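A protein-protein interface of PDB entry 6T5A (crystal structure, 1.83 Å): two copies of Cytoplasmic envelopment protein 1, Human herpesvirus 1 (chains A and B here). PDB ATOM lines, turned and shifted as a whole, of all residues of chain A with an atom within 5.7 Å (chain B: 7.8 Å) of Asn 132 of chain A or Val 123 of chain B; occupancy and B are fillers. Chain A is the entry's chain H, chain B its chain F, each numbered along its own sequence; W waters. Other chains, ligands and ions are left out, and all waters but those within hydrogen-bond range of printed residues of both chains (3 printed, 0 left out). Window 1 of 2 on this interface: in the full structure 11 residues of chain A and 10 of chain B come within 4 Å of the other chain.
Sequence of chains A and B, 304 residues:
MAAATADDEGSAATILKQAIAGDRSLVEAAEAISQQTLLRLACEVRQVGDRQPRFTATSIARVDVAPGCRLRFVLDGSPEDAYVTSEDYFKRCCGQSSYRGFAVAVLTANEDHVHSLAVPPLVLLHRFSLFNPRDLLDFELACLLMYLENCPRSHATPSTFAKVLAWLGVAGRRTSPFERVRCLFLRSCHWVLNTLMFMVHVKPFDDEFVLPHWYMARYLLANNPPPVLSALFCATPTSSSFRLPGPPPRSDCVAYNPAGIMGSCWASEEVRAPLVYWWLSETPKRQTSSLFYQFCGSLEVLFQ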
ATOM      1  N   ARG A 100     -18.510  -5.188  26.130  1.00  0.00           N
ATOM      2  CA  ARG A 100     -17.622  -6.224  26.678  1.00  0.00           C
ATOM      3  C   ARG A 100     -18.340  -7.354  27.402  1.00  0.00           C
ATOM      4  O   ARG A 100     -17.703  -8.327  27.792  1.00  0.00           O
ATOM      5  CB  ARG A 100     -16.553  -5.591  27.593  1.00  0.00           C
ATOM      6  CG  ARG A 100     -15.794  -4.398  26.990  1.00  0.00           C
ATOM      7  CD  ARG A 100     -14.843  -4.792  25.876  1.00  0.00           C
ATOM      8  NE  ARG A 100     -14.145  -3.621  25.334  1.00  0.00           N
ATOM      9  CZ  ARG A 100     -12.874  -3.326  25.579  1.00  0.00           C
ATOM     10  NH1 ARG A 100     -12.134  -4.123  26.347  1.00  0.00           N
ATOM     11  NH2 ARG A 100     -12.324  -2.241  25.051  1.00  0.00           N
ATOM     12  N   GLY A 101     -19.653  -7.224  27.563  1.00  0.00           N
ATOM     13  CA  GLY A 101     -20.489  -8.195  28.259  1.00  0.00           C
ATOM     14  C   GLY A 101     -21.038  -7.623  29.558  1.00  0.00           C
ATOM     15  O   GLY A 101     -21.100  -6.407  29.724  1.00  0.00           O
ATOM     16  N   PHE A 102     -21.424  -8.502  30.495  1.00  0.00           N
ATOM     17  CA  PHE A 102     -21.940  -8.075  31.800  1.00  0.00           C
ATOM     18  C   PHE A 102     -20.949  -8.354  32.926  1.00  0.00           C
ATOM     19  O   PHE A 102     -20.357  -9.432  32.967  1.00  0.00           O
ATOM     20  CB  PHE A 102     -23.249  -8.814  32.142  1.00  0.00           C
ATOM     21  CG  PHE A 102     -24.461  -8.438  31.328  1.00  0.00           C
ATOM     22  CD1 PHE A 102     -24.722  -9.059  30.110  1.00  0.00           C
ATOM     23  CD2 PHE A 102     -25.391  -7.532  31.819  1.00  0.00           C
ATOM     24  CE1 PHE A 102     -25.874  -8.743  29.377  1.00  0.00           C
ATOM     25  CE2 PHE A 102     -26.540  -7.214  31.083  1.00  0.00           C
ATOM     26  CZ  PHE A 102     -26.763  -7.812  29.862  1.00  0.00           C
ATOM     27  N   LEU A 130     -16.763 -11.679  34.336  1.00  0.00           N
ATOM     28  CA  LEU A 130     -17.286 -11.096  33.106  1.00  0.00           C
ATOM     29  C   LEU A 130     -18.120 -12.147  32.386  1.00  0.00           C
ATOM     30  O   LEU A 130     -17.630 -13.238  32.105  1.00  0.00           O
ATOM     31  CB  LEU A 130     -16.114 -10.638  32.206  1.00  0.00           C
ATOM     32  CG  LEU A 130     -16.489  -9.921  30.909  1.00  0.00           C
ATOM     33  CD1 LEU A 130     -17.280  -8.639  31.191  1.00  0.00           C
ATOM     34  CD2 LEU A 130     -15.247  -9.645  30.083  1.00  0.00           C
ATOM     35  N   PHE A 131     -19.370 -11.811  32.082  1.00  0.00           N
ATOM     36  CA  PHE A 131     -20.303 -12.727  31.436  1.00  0.00           C
ATOM     37  C   PHE A 131     -20.501 -12.364  29.989  1.00  0.00           C
ATOM     38  O   PHE A 131     -20.849 -11.221  29.676  1.00  0.00           O
ATOM     39  CB  PHE A 131     -21.673 -12.734  32.175  1.00  0.00           C
ATOM     40  CG  PHE A 131     -22.689 -13.749  31.682  1.00  0.00           C
ATOM     41  CD1 PHE A 131     -22.342 -15.084  31.516  1.00  0.00           C
ATOM     42  CD2 PHE A 131     -24.010 -13.376  31.448  1.00  0.00           C
ATOM     43  CE1 PHE A 131     -23.287 -16.024  31.106  1.00  0.00           C
ATOM     44  CE2 PHE A 131     -24.960 -14.322  31.061  1.00  0.00           C
ATOM     45  CZ  PHE A 131     -24.591 -15.637  30.890  1.00  0.00           C
ATOM     46  N   ASN A 132     -20.246 -13.330  29.103  1.00  0.00           N
ATOM     47  CA  ASN A 132     -20.477 -13.146  27.679  1.00  0.00           C
ATOM     48  C   ASN A 132     -21.567 -14.130  27.321  1.00  0.00           C
ATOM     49  O   ASN A 132     -21.290 -15.339  27.224  1.00  0.00           O
ATOM     50  CB  ASN A 132     -19.193 -13.339  26.850  1.00  0.00           C
ATOM     51  CG  ASN A 132     -18.147 -12.299  27.170  1.00  0.00           C
ATOM     52  OD1 ASN A 132     -17.035 -12.622  27.585  1.00  0.00           O
ATOM     53  ND2 ASN A 132     -18.483 -11.033  26.996  1.00  0.00           N
ATOM     54  N   PRO A 133     -22.835 -13.645  27.252  1.00  0.00           N
ATOM     55  CA  PRO A 133     -23.959 -14.545  26.951  1.00  0.00           C
ATOM     56  C   PRO A 133     -23.705 -15.435  25.736  1.00  0.00           C
ATOM     57  O   PRO A 133     -23.257 -14.969  24.693  1.00  0.00           O
ATOM     58  CB  PRO A 133     -25.136 -13.586  26.771  1.00  0.00           C
ATOM     59  CG  PRO A 133     -24.780 -12.424  27.622  1.00  0.00           C
ATOM     60  CD  PRO A 133     -23.306 -12.253  27.410  1.00  0.00           C
ATOM     61  N   ARG A 134     -23.899 -16.736  25.937  1.00  0.00           N
ATOM     62  CA  ARG A 134     -23.656 -17.791  24.959  1.00  0.00           C
ATOM     63  C   ARG A 134     -24.818 -17.894  23.959  1.00  0.00           C
ATOM     64  O   ARG A 134     -24.612 -18.322  22.833  1.00  0.00           O
ATOM     65  CB  ARG A 134     -23.402 -19.136  25.689  1.00  0.00           C
ATOM     66  CG  ARG A 134     -22.238 -19.101  26.708  1.00  0.00           C
ATOM     67  CD  ARG A 134     -22.275 -20.221  27.743  1.00  0.00           C
ATOM     68  NE  ARG A 134     -23.339 -20.012  28.729  1.00  0.00           N
ATOM     69  CZ  ARG A 134     -23.592 -20.796  29.776  1.00  0.00           C
ATOM     70  NH1 ARG A 134     -22.847 -21.871  30.006  1.00  0.00           N
ATOM     71  NH2 ARG A 134     -24.596 -20.513  30.597  1.00  0.00           N
ATOM     72  N   ASP A 138     -29.408 -16.764  27.986  1.00  0.00           N
ATOM     73  CA  ASP A 138     -28.342 -16.241  28.848  1.00  0.00           C
ATOM     74  C   ASP A 138     -28.422 -14.717  28.919  1.00  0.00           C
ATOM     75  O   ASP A 138     -28.274 -14.148  29.992  1.00  0.00           O
ATOM     76  CB  ASP A 138     -26.977 -16.588  28.230  1.00  0.00           C
ATOM     77  CG  ASP A 138     -26.305 -17.829  28.755  1.00  0.00           C
ATOM     78  OD1 ASP A 138     -26.970 -18.610  29.488  1.00  0.00           O
ATOM     79  OD2 ASP A 138     -25.121 -18.035  28.421  1.00  0.00           O
ATOM     80  N   GLN A 287     -14.345 -15.721  33.728  1.00  0.00           N
ATOM     81  CA  GLN A 287     -15.530 -15.771  32.873  1.00  0.00           C
ATOM     82  C   GLN A 287     -16.676 -16.341  33.691  1.00  0.00           C
ATOM     83  O   GLN A 287     -16.519 -17.401  34.293  1.00  0.00           O
ATOM     84  CB  GLN A 287     -15.265 -16.639  31.627  1.00  0.00           C
ATOM     85  CG  GLN A 287     -14.219 -16.053  30.678  1.00  0.00           C
ATOM     86  CD  GLN A 287     -13.646 -17.097  29.754  1.00  0.00           C
ATOM     87  OE1 GLN A 287     -12.475 -17.472  29.859  1.00  0.00           O
ATOM     88  NE2 GLN A 287     -14.454 -17.595  28.836  1.00  0.00           N
ATOM     89  N   THR A 288     -17.814 -15.648  33.742  1.00  0.00           N
ATOM     90  CA  THR A 288     -18.977 -16.132  34.513  1.00  0.00           C
ATOM     91  C   THR A 288     -19.383 -17.537  34.041  1.00  0.00           C
ATOM     92  O   THR A 288     -19.789 -18.367  34.856  1.00  0.00           O
ATOM     93  CB  THR A 288     -20.149 -15.173  34.394  1.00  0.00           C
ATOM     94  OG1 THR A 288     -19.698 -13.837  34.634  1.00  0.00           O
ATOM     95  CG2 THR A 288     -21.302 -15.524  35.343  1.00  0.00           C
ATOM     96  N   SER A 289     -19.243 -17.809  32.727  1.00  0.00           N
ATOM     97  CA  SER A 289     -19.616 -19.117  32.176  1.00  0.00           C
ATOM     98  C   SER A 289     -18.692 -20.268  32.654  1.00  0.00           C
ATOM     99  O   SER A 289     -19.050 -21.443  32.506  1.00  0.00           O
ATOM    100  CB  SER A 289     -19.714 -19.045  30.654  1.00  0.00           C
ATOM    101  OG  SER A 289     -18.452 -18.711  30.104  1.00  0.00           O
ATOM    102  N   VAL B 106     -12.473 -24.022  17.859  1.00  0.00           N
ATOM    103  CA  VAL B 106     -13.149 -25.266  18.220  1.00  0.00           C
ATOM    104  C   VAL B 106     -14.648 -25.003  18.306  1.00  0.00           C
ATOM    105  O   VAL B 106     -15.050 -23.999  18.877  1.00  0.00           O
ATOM    106  CB  VAL B 106     -12.536 -25.998  19.458  1.00  0.00           C
ATOM    107  CG1 VAL B 106     -12.837 -25.278  20.777  1.00  0.00           C
ATOM    108  CG2 VAL B 106     -13.015 -27.448  19.511  1.00  0.00           C
ATOM    109  N   GLU B 111     -23.219 -25.547  15.652  1.00  0.00           N
ATOM    110  CA  GLU B 111     -22.861 -24.115  15.661  1.00  0.00           C
ATOM    111  C   GLU B 111     -22.501 -23.564  14.268  1.00  0.00           C
ATOM    112  O   GLU B 111     -22.491 -22.341  14.067  1.00  0.00           O
ATOM    113  CB  GLU B 111     -21.706 -23.847  16.648  1.00  0.00           C
ATOM    114  CG  GLU B 111     -22.075 -24.029  18.115  1.00  0.00           C
ATOM    115  CD  GLU B 111     -20.908 -23.921  19.078  1.00  0.00           C
ATOM    116  OE1 GLU B 111     -19.759 -24.199  18.672  1.00  0.00           O
ATOM    117  OE2 GLU B 111     -21.139 -23.532  20.243  1.00  0.00           O
ATOM    118  N   ALA B 118     -23.084 -19.823  15.034  1.00  0.00           N
ATOM    119  CA  ALA B 118     -24.034 -19.493  16.097  1.00  0.00           C
ATOM    120  C   ALA B 118     -23.294 -19.339  17.424  1.00  0.00           C
ATOM    121  O   ALA B 118     -23.691 -19.903  18.443  1.00  0.00           O
ATOM    122  CB  ALA B 118     -25.107 -20.562  16.204  1.00  0.00           C
ATOM    123  N   VAL B 119     -22.195 -18.581  17.395  1.00  0.00           N
ATOM    124  CA  VAL B 119     -21.337 -18.328  18.540  1.00  0.00           C
ATOM    125  C   VAL B 119     -21.155 -16.811  18.611  1.00  0.00           C
ATOM    126  O   VAL B 119     -20.558 -16.255  17.686  1.00  0.00           O
ATOM    127  CB  VAL B 119     -19.963 -19.068  18.421  1.00  0.00           C
ATOM    128  CG1 VAL B 119     -19.090 -18.811  19.648  1.00  0.00           C
ATOM    129  CG2 VAL B 119     -20.146 -20.576  18.211  1.00  0.00           C
ATOM    130  N   PRO B 120     -21.657 -16.107  19.667  1.00  0.00           N
ATOM    131  CA  PRO B 120     -21.444 -14.650  19.734  1.00  0.00           C
ATOM    132  C   PRO B 120     -19.961 -14.265  19.628  1.00  0.00           C
ATOM    133  O   PRO B 120     -19.110 -15.022  20.090  1.00  0.00           O
ATOM    134  CB  PRO B 120     -22.058 -14.264  21.094  1.00  0.00           C
ATOM    135  CG  PRO B 120     -23.062 -15.334  21.361  1.00  0.00           C
ATOM    136  CD  PRO B 120     -22.422 -16.584  20.839  1.00  0.00           C
ATOM    137  N   PRO B 121     -19.613 -13.096  19.023  1.00  0.00           N
ATOM    138  CA  PRO B 121     -18.177 -12.743  18.856  1.00  0.00           C
ATOM    139  C   PRO B 121     -17.312 -12.792  20.121  1.00  0.00           C
ATOM    140  O   PRO B 121     -16.156 -13.204  20.050  1.00  0.00           O
ATOM    141  CB  PRO B 121     -18.202 -11.318  18.256  1.00  0.00           C
ATOM    142  CG  PRO B 121     -19.617 -10.909  18.218  1.00  0.00           C
ATOM    143  CD  PRO B 121     -20.499 -12.106  18.377  1.00  0.00           C
ATOM    144  N   LEU B 122     -17.859 -12.379  21.275  1.00  0.00           N
ATOM    145  CA  LEU B 122     -17.110 -12.392  22.530  1.00  0.00           C
ATOM    146  C   LEU B 122     -16.930 -13.802  23.083  1.00  0.00           C
ATOM    147  O   LEU B 122     -15.992 -14.043  23.830  1.00  0.00           O
ATOM    148  CB  LEU B 122     -17.701 -11.426  23.572  1.00  0.00           C
ATOM    149  CG  LEU B 122     -17.606  -9.937  23.180  1.00  0.00           C
ATOM    150  CD1 LEU B 122     -18.321  -9.060  24.172  1.00  0.00           C
ATOM    151  CD2 LEU B 122     -16.146  -9.482  23.034  1.00  0.00           C
ATOM    152  N   VAL B 123     -17.787 -14.740  22.671  1.00  0.00           N
ATOM    153  CA  VAL B 123     -17.670 -16.161  23.034  1.00  0.00           C
ATOM    154  C   VAL B 123     -16.643 -16.804  22.087  1.00  0.00           C
ATOM    155  O   VAL B 123     -15.792 -17.578  22.537  1.00  0.00           O
ATOM    156  CB  VAL B 123     -19.040 -16.886  22.986  1.00  0.00           C
ATOM    157  CG1 VAL B 123     -18.883 -18.387  23.250  1.00  0.00           C
ATOM    158  CG2 VAL B 123     -20.010 -16.263  23.985  1.00  0.00           C
ATOM    159  N   LEU B 124     -16.708 -16.466  20.774  1.00  0.00           N
ATOM    160  CA  LEU B 124     -15.782 -17.004  19.770  1.00  0.00           C
ATOM    161  C   LEU B 124     -14.323 -16.709  20.112  1.00  0.00           C
ATOM    162  O   LEU B 124     -13.445 -17.541  19.884  1.00  0.00           O
ATOM    163  CB  LEU B 124     -16.148 -16.531  18.345  1.00  0.00           C
ATOM    164  CG  LEU B 124     -15.437 -17.270  17.193  1.00  0.00           C
ATOM    165  CD1 LEU B 124     -15.808 -18.774  17.166  1.00  0.00           C
ATOM    166  CD2 LEU B 124     -15.753 -16.608  15.849  1.00  0.00           C
ATOM    167  N   LEU B 125     -14.088 -15.551  20.731  1.00  0.00           N
ATOM    168  CA  LEU B 125     -12.795 -15.089  21.227  1.00  0.00           C
ATOM    169  C   LEU B 125     -12.099 -16.187  22.052  1.00  0.00           C
ATOM    170  O   LEU B 125     -10.891 -16.380  21.918  1.00  0.00           O
ATOM    171  CB  LEU B 125     -13.085 -13.884  22.128  1.00  0.00           C
ATOM    172  CG  LEU B 125     -12.019 -12.829  22.291  1.00  0.00           C
ATOM    173  CD1 LEU B 125     -11.530 -12.323  20.947  1.00  0.00           C
ATOM    174  CD2 LEU B 125     -12.578 -11.659  23.091  1.00  0.00           C
ATOM    175  N   HIS B 126     -12.889 -16.932  22.864  1.00  0.00           N
ATOM    176  CA  HIS B 126     -12.435 -18.002  23.756  1.00  0.00           C
ATOM    177  C   HIS B 126     -12.401 -19.396  23.108  1.00  0.00           C
ATOM    178  O   HIS B 126     -12.026 -20.370  23.778  1.00  0.00           O
ATOM    179  CB  HIS B 126     -13.265 -18.007  25.053  1.00  0.00           C
ATOM    180  CG  HIS B 126     -13.248 -16.683  25.751  1.00  0.00           C
ATOM    181  ND1 HIS B 126     -12.112 -16.221  26.389  1.00  0.00           N
ATOM    182  CD2 HIS B 126     -14.205 -15.733  25.820  1.00  0.00           C
ATOM    183  CE1 HIS B 126     -12.423 -15.025  26.862  1.00  0.00           C
ATOM    184  NE2 HIS B 126     -13.669 -14.684  26.536  1.00  0.00           N
ATOM    185  N   ARG B 127     -12.734 -19.484  21.801  1.00  0.00           N
ATOM    186  CA  ARG B 127     -12.694 -20.760  21.067  1.00  0.00           C
ATOM    187  C   ARG B 127     -11.420 -20.942  20.252  1.00  0.00           C
ATOM    188  O   ARG B 127     -11.184 -22.037  19.728  1.00  0.00           O
ATOM    189  CB  ARG B 127     -13.935 -20.924  20.156  1.00  0.00           C
ATOM    190  CG  ARG B 127     -15.251 -20.905  20.931  1.00  0.00           C
ATOM    191  CD  ARG B 127     -15.507 -22.182  21.713  1.00  0.00           C
ATOM    192  NE  ARG B 127     -16.895 -22.218  22.171  1.00  0.00           N
ATOM    193  CZ  ARG B 127     -17.909 -22.668  21.444  1.00  0.00           C
ATOM    194  NH1 ARG B 127     -17.701 -23.150  20.224  1.00  0.00           N
ATOM    195  NH2 ARG B 127     -19.140 -22.618  21.917  1.00  0.00           N
ATOM    196  N   PHE B 128     -10.611 -19.877  20.111  1.00  0.00           N
ATOM    197  CA  PHE B 128      -9.387 -19.976  19.324  1.00  0.00           C
ATOM    198  C   PHE B 128      -8.259 -20.553  20.142  1.00  0.00           C
ATOM    199  O   PHE B 128      -8.165 -20.313  21.354  1.00  0.00           O
ATOM    200  CB  PHE B 128      -8.946 -18.608  18.756  1.00  0.00           C
ATOM    201  CG  PHE B 128      -9.914 -17.954  17.799  1.00  0.00           C
ATOM    202  CD1 PHE B 128     -10.072 -18.439  16.503  1.00  0.00           C
ATOM    203  CD2 PHE B 128     -10.682 -16.866  18.198  1.00  0.00           C
ATOM    204  CE1 PHE B 128     -10.991 -17.851  15.626  1.00  0.00           C
ATOM    205  CE2 PHE B 128     -11.590 -16.270  17.313  1.00  0.00           C
ATOM    206  CZ  PHE B 128     -11.750 -16.778  16.041  1.00  0.00           C
ATOM    207  N   PRO B 274     -13.144 -11.161  16.007  1.00  0.00           N
ATOM    208  CA  PRO B 274     -12.672 -11.916  17.184  1.00  0.00           C
ATOM    209  C   PRO B 274     -11.319 -12.606  16.967  1.00  0.00           C
ATOM    210  O   PRO B 274     -10.547 -12.695  17.918  1.00  0.00           O
ATOM    211  CB  PRO B 274     -13.777 -12.959  17.397  1.00  0.00           C
ATOM    212  CG  PRO B 274     -14.957 -12.376  16.798  1.00  0.00           C
ATOM    213  CD  PRO B 274     -14.481 -11.637  15.597  1.00  0.00           C
HETATM  214  O   HOH W   1     -14.907 -12.274  25.906  1.00  0.00           O
HETATM  215  O   HOH W   2     -26.420 -19.263  20.164  1.00  0.00           O
HETATM  216  O   HOH W   3     -10.367 -18.257  27.868  1.00  0.00           O
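The backbone carbonyl oxygen (O) of Arg 100 of chain A lies within hydrogen-bond range of the side-chain amide nitrogen (ND2) of Asn 132 of chain A (2.9 Å).
NE of Arg 134 of chain A lies within salt-bridge range of OD2 of Asp 138 of chain A, at 2.7 Å.
Among the printed residues, pairs that only touch across the chains: Pro 133 of chain A with Pro 120 of chain B, Arg 134 of chain A with Pro 120 of chain B, Gln 287 of chain A with His 126 of chain B, Asn 132 of chain A with Leu 122 of chain B, Pro 133 of chain A with Val 123 of chain B, Asn 132 of chain A with Val 123 of chain B and Arg 100 of chain A with Leu 122 of chain B.
Asn 132 of chain A touches just these residues of chain B: Leu 122 and Val 123.
Of chain A, only Asn 132 and Pro 133 come within 4 Å of Val 123 of chain B.
Of the printed residues of chain A, Pro 120 of chain B touches Pro 133 (3.4 Å) and Arg 134 (3.4 Å).
Printed residues of chain A within 4 Å of His 126 of chain B: Gln 287 (3.4 Å).
Printed residues of chain B within 4 Å of Arg 100 of chain A: Leu 122 (3.7 Å).
Printed residues of chain A within 4 Å of Leu 122 of chain B: Arg 100 and Asn 132.
Printed residues of chain B within 4 Å of Gln 287 of chain A: His 126 (3.4 Å).
Phe 128 of chain B touches none of the printed residues of chain A.
The nearest residue of chain B that does not touch Asn 132 of chain A is His 126 of chain B (4.1 Å).
The nearest residue of chain A that does not touch Val 123 of chain B is Arg 134 of chain A (4.1 Å).
The nearest printed residue of chain A that does not touch Leu 122 of chain B is Gly 101 of chain A (4.1 Å).
Of the 12 printed residues of chain A, 5 touch a printed residue of chain B.
Printed residues of chain A that touch a printed residue of chain B: Arg 100, Asn 132, Pro 133, Arg 134 and Gln 287.
Hydrophobic or aromatic side chains of chain B that line the printed part of chain A: Pro 120, Leu 122, Val 123 and His 126.
Among the printed residues, no Asp or Glu carboxylate lies within 4 Å of a Lys or Arg side-chain nitrogen of the other chain.
No position is printed for both chains.
Of the 7 pairs that touch across the chains among the printed residues, none has its exchanged pair printed and touching as well.
Water W1 lies within hydrogen-bond range of OD1 of Asn 132 of chain A, NE2 of His 126 of chain B and O of Leu 122 of chain B.
Water W3 bridges OE1 of Gln 287 of chain A and ND1 of His 126 of chain B.
Water W2 bridges O of Ala 118 of chain B (3.3 Å) and O of Arg 134 of chain A (3.4 Å).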
